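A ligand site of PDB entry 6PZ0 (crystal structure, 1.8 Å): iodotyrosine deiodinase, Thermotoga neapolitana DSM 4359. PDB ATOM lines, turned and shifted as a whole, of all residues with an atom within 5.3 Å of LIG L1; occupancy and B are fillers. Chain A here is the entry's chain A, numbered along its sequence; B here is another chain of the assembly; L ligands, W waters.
Water W1 lies within hydrogen-bond range of the side-chain carboxylate of Glu 68 and a nitrogen (N1) of LIG L1.
O of Met 41 of chain B sits at hydrogen-bond distance from NE1 of Trp 82, at 3.1 Å. OE2 of Glu 68 sits at hydrogen-bond distance from OH of Tyr 138. The backbone carbonyl oxygen (O) of Thr 89 is in hydrogen-bond range of the side-chain amino group (NZ) of Lys 92, at 2.7 Å. The backbone NH (N) of Phe 88 is in hydrogen-bond range of the backbone carbonyl oxygen (O) of Leu 83 (3.0 Å).
O3 of LG2 L2 is in hydrogen-bond range of O2 of LIG L1 (2.6 Å).
O4 of LG2 L2 sits at hydrogen-bond distance from N of Ser 39 of chain B, at 3.3 Å. The backbone NH (N) of Thr 139 is in hydrogen-bond range of an oxygen (O2) of LG2 L2, at 3.2 Å. The side-chain amino group (NZ) of Lys 92 lies within salt-bridge range of an oxygen (O1) of LIG L1 (2.7 Å). O1 of LG2 L2 sits at hydrogen-bond distance from NE of Arg 15 (2.7 Å). N of Met 41 of chain B sits at hydrogen-bond distance from O2 of LIG L1 (2.8 Å). The backbone carbonyl oxygen (O) of Ser 39 of chain B is in hydrogen-bond range of an oxygen (O4) of LG2 L2. N3 of LG2 L2 is in hydrogen-bond range of OG1 of Thr 139, at 3.0 Å. OE2 of Glu 68 is in salt-bridge range of N1 of LIG L1 (2.8 Å). An oxygen (O1) of LIG L1 lies within hydrogen-bond range of the side-chain hydroxyl (OH) of Tyr 72, at 2.6 Å. The backbone carbonyl oxygen (O) of Thr 139 is in hydrogen-bond range of a nitrogen (N1) of LIG L1 (3.3 Å).
Phe 71 touches LIG L1. CZ3 of Trp 82 touches C7 of LIG L1, 3.7 Å away. Leu 83 touches LIG L1 (CD2 to C5, 3.4 Å). CD2 of Phe 88 touches O1 of LIG L1 (3.8 Å). O of Thr 89 touches O1 of LIG L1, 3.9 Å away. Tyr 138 touches LIG L1. CA of Gly 40 of chain B touches O2 of LIG L1, 3.7 Å away. OH of Tyr 112 of chain B touches C6 of LIG L1, at 3.2 Å. Hydrophobic or aromatic side chains within 4 Å of LIG L1: Phe 71, Tyr 72, Trp 82, Leu 83, Phe 88, Tyr 138 and Tyr 112 of chain B.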
ATOM      1  N   ARG A  15      15.094  23.960  19.934  1.00  0.00           N
ATOM      2  CA  ARG A  15      14.744  22.739  19.211  1.00  0.00           C
ATOM      3  C   ARG A  15      13.231  22.591  19.096  1.00  0.00           C
ATOM      4  O   ARG A  15      12.734  21.620  18.510  1.00  0.00           O
ATOM      5  CB  ARG A  15      15.324  21.505  19.892  1.00  0.00           C
ATOM      6  CG  ARG A  15      16.832  21.506  19.957  1.00  0.00           C
ATOM      7  CD  ARG A  15      17.369  20.205  20.510  1.00  0.00           C
ATOM      8  NE  ARG A  15      18.816  20.177  20.605  1.00  0.00           N
ATOM      9  CZ  ARG A  15      19.528  20.652  21.627  1.00  0.00           C
ATOM     10  NH1 ARG A  15      18.936  21.206  22.668  1.00  0.00           N
ATOM     11  NH2 ARG A  15      20.841  20.569  21.609  1.00  0.00           N
ATOM     12  N   GLU A  68      21.224   9.305  12.257  1.00  0.00           N
ATOM     13  CA  GLU A  68      21.261   9.440  13.704  1.00  0.00           C
ATOM     14  C   GLU A  68      20.941   8.124  14.377  1.00  0.00           C
ATOM     15  O   GLU A  68      21.565   7.741  15.350  1.00  0.00           O
ATOM     16  CB  GLU A  68      20.264  10.494  14.182  1.00  0.00           C
ATOM     17  CG  GLU A  68      20.613  11.926  13.778  1.00  0.00           C
ATOM     18  CD  GLU A  68      21.836  12.485  14.466  1.00  0.00           C
ATOM     19  OE1 GLU A  68      22.582  11.727  15.146  1.00  0.00           O
ATOM     20  OE2 GLU A  68      22.040  13.714  14.293  1.00  0.00           O
ATOM     21  N   PHE A  71      23.904   6.085  14.401  1.00  0.00           N
ATOM     22  CA  PHE A  71      24.880   6.679  15.284  1.00  0.00           C
ATOM     23  C   PHE A  71      24.520   6.365  16.738  1.00  0.00           C
ATOM     24  O   PHE A  71      25.401   6.067  17.552  1.00  0.00           O
ATOM     25  CB  PHE A  71      24.957   8.198  15.018  1.00  0.00           C
ATOM     26  CG  PHE A  71      25.479   9.000  16.165  1.00  0.00           C
ATOM     27  CD1 PHE A  71      26.823   9.325  16.232  1.00  0.00           C
ATOM     28  CD2 PHE A  71      24.627   9.459  17.149  1.00  0.00           C
ATOM     29  CE1 PHE A  71      27.309  10.087  17.281  1.00  0.00           C
ATOM     30  CE2 PHE A  71      25.111  10.217  18.207  1.00  0.00           C
ATOM     31  CZ  PHE A  71      26.441  10.528  18.263  1.00  0.00           C
ATOM     32  N   TYR A  72      23.235   6.407  17.066  1.00  0.00           N
ATOM     33  CA  TYR A  72      22.813   6.206  18.456  1.00  0.00           C
ATOM     34  C   TYR A  72      23.010   4.770  18.891  1.00  0.00           C
ATOM     35  O   TYR A  72      23.185   4.482  20.078  1.00  0.00           O
ATOM     36  CB  TYR A  72      21.363   6.628  18.676  1.00  0.00           C
ATOM     37  CG  TYR A  72      21.275   8.066  19.114  1.00  0.00           C
ATOM     38  CD1 TYR A  72      21.252   9.097  18.179  1.00  0.00           C
ATOM     39  CD2 TYR A  72      21.266   8.406  20.458  1.00  0.00           C
ATOM     40  CE1 TYR A  72      21.205  10.405  18.562  1.00  0.00           C
ATOM     41  CE2 TYR A  72      21.217   9.712  20.863  1.00  0.00           C
ATOM     42  CZ  TYR A  72      21.188  10.718  19.913  1.00  0.00           C
ATOM     43  OH  TYR A  72      21.128  12.022  20.326  1.00  0.00           O
ATOM     44  N   LEU A  79      30.291  11.464  24.755  1.00  0.00           N
ATOM     45  CA  LEU A  79      29.146  11.902  23.970  1.00  0.00           C
ATOM     46  C   LEU A  79      27.910  11.056  24.246  1.00  0.00           C
ATOM     47  O   LEU A  79      26.843  11.600  24.469  1.00  0.00           O
ATOM     48  CB  LEU A  79      29.478  11.869  22.488  1.00  0.00           C
ATOM     49  CG  LEU A  79      28.412  12.428  21.554  1.00  0.00           C
ATOM     50  CD1 LEU A  79      27.950  13.817  21.962  1.00  0.00           C
ATOM     51  CD2 LEU A  79      29.001  12.438  20.157  1.00  0.00           C
ATOM     52  N   TRP A  82      26.568  11.984  27.721  1.00  0.00           N
ATOM     53  CA  TRP A  82      25.905  13.286  27.704  1.00  0.00           C
ATOM     54  C   TRP A  82      24.534  13.191  27.017  1.00  0.00           C
ATOM     55  O   TRP A  82      23.529  13.703  27.524  1.00  0.00           O
ATOM     56  CB  TRP A  82      26.803  14.313  26.989  1.00  0.00           C
ATOM     57  CG  TRP A  82      26.317  15.750  27.035  1.00  0.00           C
ATOM     58  CD1 TRP A  82      26.545  16.663  28.015  1.00  0.00           C
ATOM     59  CD2 TRP A  82      25.518  16.411  26.046  1.00  0.00           C
ATOM     60  NE1 TRP A  82      25.947  17.850  27.712  1.00  0.00           N
ATOM     61  CE2 TRP A  82      25.314  17.729  26.510  1.00  0.00           C
ATOM     62  CE3 TRP A  82      24.974  16.033  24.820  1.00  0.00           C
ATOM     63  CZ2 TRP A  82      24.594  18.659  25.794  1.00  0.00           C
ATOM     64  CZ3 TRP A  82      24.252  16.954  24.099  1.00  0.00           C
ATOM     65  CH2 TRP A  82      24.067  18.266  24.585  1.00  0.00           C
ATOM     66  N   LEU A  83      24.484  12.538  25.857  1.00  0.00           N
ATOM     67  CA  LEU A  83      23.218  12.366  25.158  1.00  0.00           C
ATOM     68  C   LEU A  83      22.210  11.568  25.971  1.00  0.00           C
ATOM     69  O   LEU A  83      21.037  11.917  26.027  1.00  0.00           O
ATOM     70  CB  LEU A  83      23.432  11.666  23.835  1.00  0.00           C
ATOM     71  CG  LEU A  83      24.214  12.474  22.799  1.00  0.00           C
ATOM     72  CD1 LEU A  83      24.532  11.602  21.620  1.00  0.00           C
ATOM     73  CD2 LEU A  83      23.466  13.738  22.348  1.00  0.00           C
ATOM     74  N   PHE A  88      18.406  12.729  24.753  1.00  0.00           N
ATOM     75  CA  PHE A  88      18.404  12.882  23.290  1.00  0.00           C
ATOM     76  C   PHE A  88      18.047  11.566  22.628  1.00  0.00           C
ATOM     77  O   PHE A  88      18.396  10.488  23.143  1.00  0.00           O
ATOM     78  CB  PHE A  88      19.783  13.329  22.792  1.00  0.00           C
ATOM     79  CG  PHE A  88      20.066  14.803  22.970  1.00  0.00           C
ATOM     80  CD1 PHE A  88      20.312  15.349  24.212  1.00  0.00           C
ATOM     81  CD2 PHE A  88      20.099  15.624  21.869  1.00  0.00           C
ATOM     82  CE1 PHE A  88      20.575  16.701  24.363  1.00  0.00           C
ATOM     83  CE2 PHE A  88      20.372  16.969  22.007  1.00  0.00           C
ATOM     84  CZ  PHE A  88      20.606  17.513  23.257  1.00  0.00           C
ATOM     85  N   THR A  89      17.415  11.610  21.449  1.00  0.00           N
ATOM     86  CA  THR A  89      17.323  10.409  20.635  1.00  0.00           C
ATOM     87  C   THR A  89      17.551  10.775  19.185  1.00  0.00           C
ATOM     88  O   THR A  89      17.820  11.914  18.880  1.00  0.00           O
ATOM     89  CB  THR A  89      15.973   9.692  20.741  1.00  0.00           C
ATOM     90  OG1 THR A  89      14.996  10.383  19.968  1.00  0.00           O
ATOM     91  CG2 THR A  89      15.521   9.620  22.187  1.00  0.00           C
ATOM     92  N   LYS A  92      14.327  13.673  14.961  1.00  0.00           N
ATOM     93  CA  LYS A  92      14.615  15.104  14.778  1.00  0.00           C
ATOM     94  C   LYS A  92      13.431  15.824  14.192  1.00  0.00           C
ATOM     95  O   LYS A  92      13.482  16.314  13.058  1.00  0.00           O
ATOM     96  CB  LYS A  92      15.825  15.278  13.871  1.00  0.00           C
ATOM     97  CG  LYS A  92      17.087  14.604  14.370  1.00  0.00           C
ATOM     98  CD  LYS A  92      17.519  15.099  15.781  1.00  0.00           C
ATOM     99  CE  LYS A  92      18.450  14.140  16.463  1.00  0.00           C
ATOM    100  NZ  LYS A  92      18.501  14.382  17.984  1.00  0.00           N
ATOM    101  N   TYR A 138      22.663  22.061  13.853  1.00  0.00           N
ATOM    102  CA  TYR A 138      22.399  20.636  13.764  1.00  0.00           C
ATOM    103  C   TYR A 138      23.397  19.991  12.831  1.00  0.00           C
ATOM    104  O   TYR A 138      23.536  20.377  11.678  1.00  0.00           O
ATOM    105  CB  TYR A 138      20.965  20.378  13.310  1.00  0.00           C
ATOM    106  CG  TYR A 138      20.785  18.905  13.129  1.00  0.00           C
ATOM    107  CD1 TYR A 138      20.927  18.037  14.201  1.00  0.00           C
ATOM    108  CD2 TYR A 138      20.545  18.377  11.875  1.00  0.00           C
ATOM    109  CE1 TYR A 138      20.805  16.669  14.021  1.00  0.00           C
ATOM    110  CE2 TYR A 138      20.430  17.036  11.688  1.00  0.00           C
ATOM    111  CZ  TYR A 138      20.553  16.176  12.773  1.00  0.00           C
ATOM    112  OH  TYR A 138      20.468  14.828  12.587  1.00  0.00           O
ATOM    113  N   THR A 139      24.080  18.966  13.346  1.00  0.00           N
ATOM    114  CA  THR A 139      25.139  18.304  12.613  1.00  0.00           C
ATOM    115  C   THR A 139      24.900  16.798  12.646  1.00  0.00           C
ATOM    116  O   THR A 139      25.299  16.142  13.585  1.00  0.00           O
ATOM    117  CB  THR A 139      26.521  18.625  13.220  1.00  0.00           C
ATOM    118  OG1 THR A 139      26.536  18.233  14.597  1.00  0.00           O
ATOM    119  CG2 THR A 139      26.820  20.118  13.145  1.00  0.00           C
ATOM    120  N   PRO A 140      24.231  16.252  11.627  1.00  0.00           N
ATOM    121  CA  PRO A 140      24.030  14.798  11.580  1.00  0.00           C
ATOM    122  C   PRO A 140      25.339  14.067  11.333  1.00  0.00           C
ATOM    123  O   PRO A 140      26.304  14.684  10.911  1.00  0.00           O
ATOM    124  CB  PRO A 140      23.079  14.609  10.396  1.00  0.00           C
ATOM    125  CG  PRO A 140      23.400  15.776   9.499  1.00  0.00           C
ATOM    126  CD  PRO A 140      23.752  16.917  10.410  1.00  0.00           C
ATOM    127  N   PRO A 141      25.379  12.755  11.587  1.00  0.00           N
ATOM    128  CA  PRO A 141      26.609  11.979  11.463  1.00  0.00           C
ATOM    129  C   PRO A 141      27.192  12.005  10.062  1.00  0.00           C
ATOM    130  O   PRO A 141      28.411  11.972   9.902  1.00  0.00           O
ATOM    131  CB  PRO A 141      26.182  10.557  11.823  1.00  0.00           C
ATOM    132  CG  PRO A 141      24.955  10.701  12.626  1.00  0.00           C
ATOM    133  CD  PRO A 141      24.268  11.956  12.147  1.00  0.00           C
ATOM    134  N   SER B  39      28.221  24.926  21.949  1.00  0.00           N
ATOM    135  CA  SER B  39      29.309  24.037  21.558  1.00  0.00           C
ATOM    136  C   SER B  39      28.735  22.627  21.524  1.00  0.00           C
ATOM    137  O   SER B  39      27.701  22.369  22.148  1.00  0.00           O
ATOM    138  CB  SER B  39      30.484  24.104  22.541  1.00  0.00           C
ATOM    139  OG  SER B  39      30.098  23.705  23.850  1.00  0.00           O
ATOM    140  N   GLY B  40      29.387  21.752  20.768  1.00  0.00           N
ATOM    141  CA  GLY B  40      28.969  20.369  20.650  1.00  0.00           C
ATOM    142  C   GLY B  40      28.958  19.759  22.061  1.00  0.00           C
ATOM    143  O   GLY B  40      29.915  19.900  22.812  1.00  0.00           O
ATOM    144  N   MET B  41      27.879  19.042  22.359  1.00  0.00           N
ATOM    145  CA  MET B  41      27.597  18.494  23.696  1.00  0.00           C
ATOM    146  C   MET B  41      27.928  19.436  24.863  1.00  0.00           C
ATOM    147  O   MET B  41      28.226  18.976  26.010  1.00  0.00           O
ATOM    148  CB  MET B  41      28.291  17.139  23.886  1.00  0.00           C
ATOM    149  CG  MET B  41      29.805  17.102  23.815  1.00  0.00           C
ATOM    150  SD  MET B  41      30.390  15.487  24.490  1.00  0.00           S
ATOM    151  CE  MET B  41      30.304  15.836  26.221  1.00  0.00           C
ATOM    152  N   ASN B  42      27.770  20.732  24.624  1.00  0.00           N
ATOM    153  CA  ASN B  42      28.081  21.767  25.607  1.00  0.00           C
ATOM    154  C   ASN B  42      29.453  21.544  26.265  1.00  0.00           C
ATOM    155  O   ASN B  42      29.658  21.808  27.456  1.00  0.00           O
ATOM    156  CB  ASN B  42      26.988  21.874  26.672  1.00  0.00           C
ATOM    157  CG  ASN B  42      27.086  23.172  27.484  1.00  0.00           C
ATOM    158  OD1 ASN B  42      27.453  24.219  26.959  1.00  0.00           O
ATOM    159  ND2 ASN B  42      26.780  23.079  28.771  1.00  0.00           N
ATOM    160  N   TYR B 112      33.130  17.888  17.984  1.00  0.00           N
ATOM    161  CA  TYR B 112      32.805  19.159  17.360  1.00  0.00           C
ATOM    162  C   TYR B 112      33.639  20.304  17.923  1.00  0.00           C
ATOM    163  O   TYR B 112      33.186  21.463  17.923  1.00  0.00           O
ATOM    164  CB  TYR B 112      31.330  19.482  17.555  1.00  0.00           C
ATOM    165  CG  TYR B 112      30.435  18.285  17.394  1.00  0.00           C
ATOM    166  CD1 TYR B 112      30.033  17.891  16.139  1.00  0.00           C
ATOM    167  CD2 TYR B 112      30.016  17.531  18.495  1.00  0.00           C
ATOM    168  CE1 TYR B 112      29.230  16.764  15.965  1.00  0.00           C
ATOM    169  CE2 TYR B 112      29.213  16.407  18.334  1.00  0.00           C
ATOM    170  CZ  TYR B 112      28.818  16.037  17.059  1.00  0.00           C
ATOM    171  OH  TYR B 112      28.029  14.925  16.873  1.00  0.00           O
HETATM  172  N1  LIG L   1      23.730  14.876  16.240  1.00  0.00           N
HETATM  173  C1  LIG L   1      23.152  14.063  17.323  1.00  0.00           C
HETATM  174  C2  LIG L   1      21.770  14.579  17.714  1.00  0.00           C
HETATM  175  O1  LIG L   1      21.090  13.969  18.544  1.00  0.00           O
HETATM  176  C3  LIG L   1      24.087  14.036  18.534  1.00  0.00           C
HETATM  177  C4  LIG L   1      24.464  15.380  19.123  1.00  0.00           C
HETATM  178  C5  LIG L   1      23.563  16.095  19.904  1.00  0.00           C
HETATM  179  C6  LIG L   1      25.727  15.908  18.927  1.00  0.00           C
HETATM  180  C7  LIG L   1      23.920  17.317  20.466  1.00  0.00           C
HETATM  181  C8  LIG L   1      26.093  17.126  19.512  1.00  0.00           C
HETATM  182  C9  LIG L   1      25.177  17.819  20.256  1.00  0.00           C
HETATM  183  O2  LIG L   1      25.541  19.027  20.800  1.00  0.00           O
HETATM  184  O3  LIG L   1      21.339  15.622  17.210  1.00  0.00           O
HETATM  185  N1  LG2 L   2      22.417  20.053  19.052  1.00  0.00           N
HETATM  186  C1  LG2 L   2      21.693  18.992  18.640  1.00  0.00           C
HETATM  187  O1  LG2 L   2      20.612  18.775  19.138  1.00  0.00           O
HETATM  188  N2  LG2 L   2      22.192  18.173  17.676  1.00  0.00           N
HETATM  189  C2  LG2 L   2      23.403  18.398  17.078  1.00  0.00           C
HETATM  190  O2  LG2 L   2      23.808  17.628  16.206  1.00  0.00           O
HETATM  191  C3  LG2 L   2      24.147  19.494  17.502  1.00  0.00           C
HETATM  192  N3  LG2 L   2      25.377  19.757  16.930  1.00  0.00           N
HETATM  193  C4  LG2 L   2      26.093  20.862  17.331  1.00  0.00           C
HETATM  194  C5  LG2 L   2      27.323  21.119  16.731  1.00  0.00           C
HETATM  195  C6  LG2 L   2      28.073  22.231  17.108  1.00  0.00           C
HETATM  196  C7  LG2 L   2      29.388  22.481  16.427  1.00  0.00           C
HETATM  197  C8  LG2 L   2      27.569  23.073  18.095  1.00  0.00           C
HETATM  198  C9  LG2 L   2      28.364  24.279  18.475  1.00  0.00           C
HETATM  199  C10 LG2 L   2      26.339  22.819  18.708  1.00  0.00           C
HETATM  200  C11 LG2 L   2      25.589  21.708  18.332  1.00  0.00           C
HETATM  201  N4  LG2 L   2      24.350  21.416  18.933  1.00  0.00           N
HETATM  202  C12 LG2 L   2      23.638  20.319  18.479  1.00  0.00           C
HETATM  203  C13 LG2 L   2      23.780  22.297  20.000  1.00  0.00           C
HETATM  204  C14 LG2 L   2      24.475  22.010  21.356  1.00  0.00           C
HETATM  205  O3  LG2 L   2      23.975  20.820  21.949  1.00  0.00           O
HETATM  206  C15 LG2 L   2      24.300  23.196  22.298  1.00  0.00           C
HETATM  207  O4  LG2 L   2      25.000  24.281  21.740  1.00  0.00           O
HETATM  208  C16 LG2 L   2      24.815  22.941  23.730  1.00  0.00           C
HETATM  209  O5  LG2 L   2      24.031  21.931  24.314  1.00  0.00           O
HETATM  210  C17 LG2 L   2      24.700  24.180  24.562  1.00  0.00           C
HETATM  211  O6  LG2 L   2      23.359  24.626  24.525  1.00  0.00           O
HETATM  212  P1  LG2 L   2      22.935  25.905  25.333  1.00  0.00           P
HETATM  213  O7  LG2 L   2      21.413  26.038  25.212  1.00  0.00           O
HETATM  214  O8  LG2 L   2      23.589  27.126  24.727  1.00  0.00           O
HETATM  215  O9  LG2 L   2      23.400  25.778  26.770  1.00  0.00           O
HETATM  216  O   HOH W   1      25.138  12.444  15.629  1.00  0.00           O
